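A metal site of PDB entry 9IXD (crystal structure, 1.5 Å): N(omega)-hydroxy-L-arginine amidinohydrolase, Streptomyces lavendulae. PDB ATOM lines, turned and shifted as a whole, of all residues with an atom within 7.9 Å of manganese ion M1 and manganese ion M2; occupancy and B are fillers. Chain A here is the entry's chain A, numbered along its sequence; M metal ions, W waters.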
ATOM      1  N   THR A  85     -24.929  30.147 -17.208  1.00  0.00           N
ATOM      2  CA  THR A  85     -25.971  29.145 -17.407  1.00  0.00           C
ATOM      3  C   THR A  85     -26.404  29.079 -18.874  1.00  0.00           C
ATOM      4  O   THR A  85     -26.196  30.008 -19.658  1.00  0.00           O
ATOM      5  CB  THR A  85     -27.219  29.427 -16.562  1.00  0.00           C
ATOM      6  OG1 THR A  85     -27.820  30.666 -16.986  1.00  0.00           O
ATOM      7  CG2 THR A  85     -26.899  29.488 -15.085  1.00  0.00           C
ATOM      8  N   CYS A  86     -27.001  27.932 -19.239  1.00  0.00           N
ATOM      9  CA  CYS A  86     -27.566  27.815 -20.569  1.00  0.00           C
ATOM     10  C   CYS A  86     -28.620  28.883 -20.834  1.00  0.00           C
ATOM     11  O   CYS A  86     -28.847  29.237 -21.995  1.00  0.00           O
ATOM     12  CB  CYS A  86     -28.195  26.423 -20.775  1.00  0.00           C
ATOM     13  SG  CYS A  86     -26.969  25.093 -20.974  1.00  0.00           S
ATOM     14  N   SER A  87     -29.289  29.375 -19.778  1.00  0.00           N
ATOM     15  CA  SER A  87     -30.383  30.329 -19.957  1.00  0.00           C
ATOM     16  C   SER A  87     -29.927  31.639 -20.582  1.00  0.00           C
ATOM     17  O   SER A  87     -30.758  32.333 -21.164  1.00  0.00           O
ATOM     18  CB  SER A  87     -31.079  30.590 -18.619  1.00  0.00           C
ATOM     19  OG  SER A  87     -31.693  29.413 -18.155  1.00  0.00           O
ATOM     20  N   TYR A 107     -26.608  21.974 -30.116  1.00  0.00           N
ATOM     21  CA  TYR A 107     -26.891  22.206 -28.703  1.00  0.00           C
ATOM     22  C   TYR A 107     -26.365  20.977 -27.956  1.00  0.00           C
ATOM     23  O   TYR A 107     -27.019  19.923 -27.924  1.00  0.00           O
ATOM     24  CB  TYR A 107     -28.385  22.436 -28.524  1.00  0.00           C
ATOM     25  CG  TYR A 107     -28.754  23.104 -27.232  1.00  0.00           C
ATOM     26  CD1 TYR A 107     -28.829  22.380 -26.050  1.00  0.00           C
ATOM     27  CD2 TYR A 107     -29.032  24.464 -27.179  1.00  0.00           C
ATOM     28  CE1 TYR A 107     -29.159  22.989 -24.845  1.00  0.00           C
ATOM     29  CE2 TYR A 107     -29.369  25.097 -25.994  1.00  0.00           C
ATOM     30  CZ  TYR A 107     -29.443  24.351 -24.808  1.00  0.00           C
ATOM     31  OH  TYR A 107     -29.764  24.973 -23.611  1.00  0.00           O
ATOM     32  N   ILE A 108     -25.163  21.094 -27.400  1.00  0.00           N
ATOM     33  CA  ILE A 108     -24.432  19.958 -26.856  1.00  0.00           C
ATOM     34  C   ILE A 108     -24.687  19.924 -25.361  1.00  0.00           C
ATOM     35  O   ILE A 108     -24.264  20.835 -24.642  1.00  0.00           O
ATOM     36  CB  ILE A 108     -22.944  20.047 -27.207  1.00  0.00           C
ATOM     37  CG1 ILE A 108     -22.786  20.239 -28.728  1.00  0.00           C
ATOM     38  CG2 ILE A 108     -22.184  18.804 -26.712  1.00  0.00           C
ATOM     39  CD1 ILE A 108     -21.348  20.265 -29.201  1.00  0.00           C
ATOM     40  N   ASP A 109     -25.408  18.907 -24.884  1.00  0.00           N
ATOM     41  CA  ASP A 109     -25.975  18.968 -23.539  1.00  0.00           C
ATOM     42  C   ASP A 109     -26.379  17.558 -23.144  1.00  0.00           C
ATOM     43  O   ASP A 109     -26.866  16.798 -23.989  1.00  0.00           O
ATOM     44  CB  ASP A 109     -27.178  19.923 -23.573  1.00  0.00           C
ATOM     45  CG  ASP A 109     -27.591  20.435 -22.227  1.00  0.00           C
ATOM     46  OD1 ASP A 109     -27.674  19.661 -21.238  1.00  0.00           O
ATOM     47  OD2 ASP A 109     -27.858  21.648 -22.158  1.00  0.00           O
ATOM     48  N   GLY A 110     -26.183  17.189 -21.881  1.00  0.00           N
ATOM     49  CA  GLY A 110     -26.726  15.926 -21.419  1.00  0.00           C
ATOM     50  C   GLY A 110     -28.240  15.906 -21.349  1.00  0.00           C
ATOM     51  O   GLY A 110     -28.851  14.829 -21.335  1.00  0.00           O
ATOM     52  N   HIS A 111     -28.864  17.086 -21.344  1.00  0.00           N
ATOM     53  CA  HIS A 111     -30.306  17.269 -21.316  1.00  0.00           C
ATOM     54  C   HIS A 111     -30.825  17.764 -22.655  1.00  0.00           C
ATOM     55  O   HIS A 111     -30.070  18.193 -23.533  1.00  0.00           O
ATOM     56  CB  HIS A 111     -30.697  18.295 -20.249  1.00  0.00           C
ATOM     57  CG  HIS A 111     -30.202  17.965 -18.876  1.00  0.00           C
ATOM     58  ND1 HIS A 111     -28.987  18.396 -18.419  1.00  0.00           N
ATOM     59  CD2 HIS A 111     -30.768  17.250 -17.879  1.00  0.00           C
ATOM     60  CE1 HIS A 111     -28.816  17.967 -17.176  1.00  0.00           C
ATOM     61  NE2 HIS A 111     -29.883  17.276 -16.819  1.00  0.00           N
ATOM     62  N   GLY A 112     -32.153  17.748 -22.801  1.00  0.00           N
ATOM     63  CA  GLY A 112     -32.755  18.340 -23.980  1.00  0.00           C
ATOM     64  C   GLY A 112     -33.051  19.834 -23.886  1.00  0.00           C
ATOM     65  O   GLY A 112     -33.202  20.512 -24.920  1.00  0.00           O
ATOM     66  N   ASP A 113     -33.119  20.366 -22.664  1.00  0.00           N
ATOM     67  CA  ASP A 113     -33.443  21.773 -22.394  1.00  0.00           C
ATOM     68  C   ASP A 113     -34.653  22.228 -23.232  1.00  0.00           C
ATOM     69  O   ASP A 113     -34.691  23.340 -23.758  1.00  0.00           O
ATOM     70  CB  ASP A 113     -32.222  22.678 -22.606  1.00  0.00           C
ATOM     71  CG  ASP A 113     -31.163  22.494 -21.509  1.00  0.00           C
ATOM     72  OD1 ASP A 113     -31.361  21.629 -20.631  1.00  0.00           O
ATOM     73  OD2 ASP A 113     -30.127  23.236 -21.530  1.00  0.00           O
ATOM     74  N   TYR A 124     -37.460  25.158 -13.649  1.00  0.00           N
ATOM     75  CA  TYR A 124     -36.144  25.731 -13.883  1.00  0.00           C
ATOM     76  C   TYR A 124     -36.016  26.277 -15.307  1.00  0.00           C
ATOM     77  O   TYR A 124     -36.199  25.546 -16.291  1.00  0.00           O
ATOM     78  CB  TYR A 124     -35.049  24.691 -13.607  1.00  0.00           C
ATOM     79  CG  TYR A 124     -33.638  25.158 -13.834  1.00  0.00           C
ATOM     80  CD1 TYR A 124     -33.209  26.399 -13.376  1.00  0.00           C
ATOM     81  CD2 TYR A 124     -32.733  24.357 -14.518  1.00  0.00           C
ATOM     82  CE1 TYR A 124     -31.905  26.831 -13.586  1.00  0.00           C
ATOM     83  CE2 TYR A 124     -31.442  24.784 -14.748  1.00  0.00           C
ATOM     84  CZ  TYR A 124     -31.026  26.020 -14.285  1.00  0.00           C
ATOM     85  OH  TYR A 124     -29.744  26.435 -14.531  1.00  0.00           O
ATOM     86  N   GLY A 126     -33.422  27.008 -16.974  1.00  0.00           N
ATOM     87  CA  GLY A 126     -32.372  26.364 -17.742  1.00  0.00           C
ATOM     88  C   GLY A 126     -32.810  25.102 -18.433  1.00  0.00           C
ATOM     89  O   GLY A 126     -32.115  24.634 -19.342  1.00  0.00           O
ATOM     90  N   GLY A 127     -33.946  24.527 -18.042  1.00  0.00           N
ATOM     91  CA  GLY A 127     -34.474  23.400 -18.764  1.00  0.00           C
ATOM     92  C   GLY A 127     -35.441  23.767 -19.863  1.00  0.00           C
ATOM     93  O   GLY A 127     -36.059  22.869 -20.424  1.00  0.00           O
ATOM     94  N   MET A 128     -35.550  25.061 -20.172  1.00  0.00           N
ATOM     95  CA  MET A 128     -36.536  25.605 -21.116  1.00  0.00           C
ATOM     96  C   MET A 128     -35.875  26.415 -22.221  1.00  0.00           C
ATOM     97  O   MET A 128     -36.553  27.170 -22.942  1.00  0.00           O
ATOM     98  CB  MET A 128     -37.553  26.459 -20.357  1.00  0.00           C
ATOM     99  CG  MET A 128     -38.172  25.757 -19.154  1.00  0.00           C
ATOM    100  SD  MET A 128     -39.010  26.835 -17.957  1.00  0.00           S
ATOM    101  CE  MET A 128     -40.352  27.404 -18.972  1.00  0.00           C
ATOM    102  N   VAL A 129     -34.561  26.281 -22.414  1.00  0.00           N
ATOM    103  CA  VAL A 129     -33.802  27.223 -23.232  1.00  0.00           C
ATOM    104  C   VAL A 129     -34.042  26.986 -24.701  1.00  0.00           C
ATOM    105  O   VAL A 129     -34.323  27.917 -25.461  1.00  0.00           O
ATOM    106  CB  VAL A 129     -32.302  27.117 -22.893  1.00  0.00           C
ATOM    107  CG1 VAL A 129     -31.467  28.013 -23.833  1.00  0.00           C
ATOM    108  CG2 VAL A 129     -32.057  27.468 -21.423  1.00  0.00           C
ATOM    109  N   LEU A 130     -33.874  25.749 -25.161  1.00  0.00           N
ATOM    110  CA  LEU A 130     -33.952  25.493 -26.593  1.00  0.00           C
ATOM    111  C   LEU A 130     -35.386  25.613 -27.072  1.00  0.00           C
ATOM    112  O   LEU A 130     -35.628  26.116 -28.166  1.00  0.00           O
ATOM    113  CB  LEU A 130     -33.351  24.114 -26.900  1.00  0.00           C
ATOM    114  CG  LEU A 130     -33.242  23.680 -28.363  1.00  0.00           C
ATOM    115  CD1 LEU A 130     -32.459  24.711 -29.177  1.00  0.00           C
ATOM    116  CD2 LEU A 130     -32.604  22.302 -28.487  1.00  0.00           C
ATOM    117  N   SER A 155     -27.346  14.298 -25.691  1.00  0.00           N
ATOM    118  CA  SER A 155     -28.477  14.209 -24.774  1.00  0.00           C
ATOM    119  C   SER A 155     -28.870  12.753 -24.559  1.00  0.00           C
ATOM    120  O   SER A 155     -28.788  11.930 -25.487  1.00  0.00           O
ATOM    121  CB  SER A 155     -29.661  14.992 -25.351  1.00  0.00           C
ATOM    122  OG  SER A 155     -29.236  16.281 -25.763  1.00  0.00           O
ATOM    123  N   HIS A 196     -23.271  25.414 -28.992  1.00  0.00           N
ATOM    124  CA  HIS A 196     -23.638  25.721 -27.610  1.00  0.00           C
ATOM    125  C   HIS A 196     -23.301  24.489 -26.770  1.00  0.00           C
ATOM    126  O   HIS A 196     -23.773  23.396 -27.060  1.00  0.00           O
ATOM    127  CB  HIS A 196     -25.137  26.053 -27.545  1.00  0.00           C
ATOM    128  CG  HIS A 196     -25.704  26.084 -26.160  1.00  0.00           C
ATOM    129  ND1 HIS A 196     -26.119  27.258 -25.566  1.00  0.00           N
ATOM    130  CD2 HIS A 196     -25.890  25.108 -25.246  1.00  0.00           C
ATOM    131  CE1 HIS A 196     -26.549  27.000 -24.338  1.00  0.00           C
ATOM    132  NE2 HIS A 196     -26.402  25.698 -24.111  1.00  0.00           N
ATOM    133  N   ILE A 197     -22.470  24.628 -25.726  1.00  0.00           N
ATOM    134  CA  ILE A 197     -22.084  23.488 -24.903  1.00  0.00           C
ATOM    135  C   ILE A 197     -22.426  23.710 -23.444  1.00  0.00           C
ATOM    136  O   ILE A 197     -22.029  24.734 -22.867  1.00  0.00           O
ATOM    137  CB  ILE A 197     -20.584  23.163 -25.005  1.00  0.00           C
ATOM    138  CG1 ILE A 197     -20.208  22.846 -26.440  1.00  0.00           C
ATOM    139  CG2 ILE A 197     -20.238  21.944 -24.124  1.00  0.00           C
ATOM    140  CD1 ILE A 197     -18.688  22.820 -26.632  1.00  0.00           C
ATOM    141  N   ASP A 198     -23.139  22.750 -22.861  1.00  0.00           N
ATOM    142  CA  ASP A 198     -23.356  22.621 -21.424  1.00  0.00           C
ATOM    143  C   ASP A 198     -22.469  21.474 -20.944  1.00  0.00           C
ATOM    144  O   ASP A 198     -22.621  20.348 -21.414  1.00  0.00           O
ATOM    145  CB  ASP A 198     -24.843  22.300 -21.220  1.00  0.00           C
ATOM    146  CG  ASP A 198     -25.253  21.981 -19.788  1.00  0.00           C
ATOM    147  OD1 ASP A 198     -24.416  21.713 -18.899  1.00  0.00           O
ATOM    148  OD2 ASP A 198     -26.493  21.962 -19.559  1.00  0.00           O
ATOM    149  N   TRP A 199     -21.527  21.784 -20.020  1.00  0.00           N
ATOM    150  CA  TRP A 199     -20.540  20.782 -19.628  1.00  0.00           C
ATOM    151  C   TRP A 199     -21.135  19.566 -18.939  1.00  0.00           C
ATOM    152  O   TRP A 199     -20.444  18.553 -18.828  1.00  0.00           O
ATOM    153  CB  TRP A 199     -19.434  21.426 -18.752  1.00  0.00           C
ATOM    154  CG  TRP A 199     -18.687  22.501 -19.487  1.00  0.00           C
ATOM    155  CD1 TRP A 199     -18.571  23.830 -19.118  1.00  0.00           C
ATOM    156  CD2 TRP A 199     -17.948  22.376 -20.720  1.00  0.00           C
ATOM    157  NE1 TRP A 199     -17.844  24.518 -20.041  1.00  0.00           N
ATOM    158  CE2 TRP A 199     -17.441  23.655 -21.039  1.00  0.00           C
ATOM    159  CE3 TRP A 199     -17.680  21.311 -21.585  1.00  0.00           C
ATOM    160  CZ2 TRP A 199     -16.680  23.909 -22.179  1.00  0.00           C
ATOM    161  CZ3 TRP A 199     -16.925  21.566 -22.741  1.00  0.00           C
ATOM    162  CH2 TRP A 199     -16.438  22.857 -23.015  1.00  0.00           C
ATOM    163  N   ASP A 200     -22.418  19.579 -18.551  1.00  0.00           N
ATOM    164  CA  ASP A 200     -22.962  18.337 -18.019  1.00  0.00           C
ATOM    165  C   ASP A 200     -23.131  17.256 -19.102  1.00  0.00           C
ATOM    166  O   ASP A 200     -23.476  16.130 -18.769  1.00  0.00           O
ATOM    167  CB  ASP A 200     -24.297  18.550 -17.246  1.00  0.00           C
ATOM    168  CG  ASP A 200     -25.483  19.036 -18.121  1.00  0.00           C
ATOM    169  OD1 ASP A 200     -25.543  18.705 -19.324  1.00  0.00           O
ATOM    170  OD2 ASP A 200     -26.396  19.730 -17.572  1.00  0.00           O
ATOM    171  N   VAL A 201     -22.823  17.554 -20.369  1.00  0.00           N
ATOM    172  CA  VAL A 201     -22.792  16.525 -21.385  1.00  0.00           C
ATOM    173  C   VAL A 201     -21.659  15.527 -21.138  1.00  0.00           C
ATOM    174  O   VAL A 201     -21.719  14.389 -21.606  1.00  0.00           O
ATOM    175  CB  VAL A 201     -22.673  17.166 -22.780  1.00  0.00           C
ATOM    176  CG1 VAL A 201     -21.251  17.681 -23.020  1.00  0.00           C
ATOM    177  CG2 VAL A 201     -23.118  16.179 -23.879  1.00  0.00           C
ATOM    178  N   ALA A 240     -20.971  26.916 -21.399  1.00  0.00           N
ATOM    179  CA  ALA A 240     -21.872  27.147 -20.278  1.00  0.00           C
ATOM    180  C   ALA A 240     -21.782  26.069 -19.214  1.00  0.00           C
ATOM    181  O   ALA A 240     -21.536  24.882 -19.507  1.00  0.00           O
ATOM    182  CB  ALA A 240     -23.345  27.276 -20.748  1.00  0.00           C
ATOM    183  N   GLU A 241     -22.021  26.486 -17.969  1.00  0.00           N
ATOM    184  CA  GLU A 241     -22.319  25.607 -16.841  1.00  0.00           C
ATOM    185  C   GLU A 241     -21.108  24.796 -16.374  1.00  0.00           C
ATOM    186  O   GLU A 241     -21.176  23.590 -16.148  1.00  0.00           O
ATOM    187  CB  GLU A 241     -23.523  24.711 -17.151  1.00  0.00           C
ATOM    188  CG  GLU A 241     -24.735  25.522 -17.691  1.00  0.00           C
ATOM    189  CD  GLU A 241     -26.093  25.139 -17.101  1.00  0.00           C
ATOM    190  OE1 GLU A 241     -26.194  24.108 -16.389  1.00  0.00           O
ATOM    191  OE2 GLU A 241     -27.083  25.868 -17.371  1.00  0.00           O
HETATM  192 MN    MN M   1     -28.254  23.025 -20.478  1.00  0.00          MN
HETATM  193 MN    MN M   2     -27.644  19.952 -19.189  1.00  0.00          MN
HETATM  194  O   HOH W   1     -29.162  24.084 -18.598  1.00  0.00           O
HETATM  195  O   HOH W   2     -29.186  21.362 -19.140  1.00  0.00           O
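OD1 of Asp 200 sits close to N of Gly 110, 3.0 Å away. The side-chain hydroxyl (OG) of Ser 155 sits at hydrogen-bond distance from the backbone carbonyl oxygen (O) of Asp 109 (3.0 Å). The backbone carbonyl oxygen (O) of Asp 113 sits at hydrogen-bond distance from the backbone NH (N) of Val 129, 3.2 Å away. The backbone NH of Leu 130 is in hydrogen-bond range of the backbone carbonyl oxygen of Asp 113, at 2.9 Å. OG of Ser 155 sits at hydrogen-bond distance from O of His 111 (3.1 Å). The backbone NH (N) of Asp 198 lies within hydrogen-bond range of the backbone carbonyl oxygen (O) of Ile 108 (2.8 Å). A ring nitrogen (NE2) of His 196 lies close to the side-chain sulfur (SG) of Cys 86 (3.2 Å). NE2 of His 196 sits close to OH of Tyr 107, at 3.5 Å.
Residues that only touch manganese ion M1: Tyr 107 (3.99 Å). Of the 25 residues printed, 5 come within 4 Å of manganese ion M1. The nearest printed residue that does not touch manganese ion M1 is Gly 126 (4.3 Å).
Within 4 Å of manganese ion M2: Asp 109, His 111, Asp 198 and Asp 200. Along chain A the residues within 4 Å of manganese ion M2 span positions 109 to 200.
Manganese ion M1 is bound by OD2 of Asp 113, at 2.2 Å. Manganese ion M1 is bound by the side-chain carboxylate (OD2) of Asp 109 (2.2 Å). OD2 of Asp 198 is bound to manganese ion M1, 2.3 Å away. Water W2 is bound to manganese ion M1 (2.3 Å). Manganese ion M1 is bound by water W1, 2.3 Å away. SG of Cys 86 is bound to manganese ion M1.
Manganese ion M2 is bound by the side-chain carboxylate (OD2) of Asp 200, the side-chain carboxylate (OD1) of Asp 109, water W2, a ring nitrogen (ND1) of His 111, the side-chain carboxylate (OD2) of Asp 198 and the side-chain carboxylate (OD1) of Asp 200.
Water W1 lies within hydrogen-bond range of OE2 of Glu 241 (3.0 Å) and O of Gly 126 (3.1 Å).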
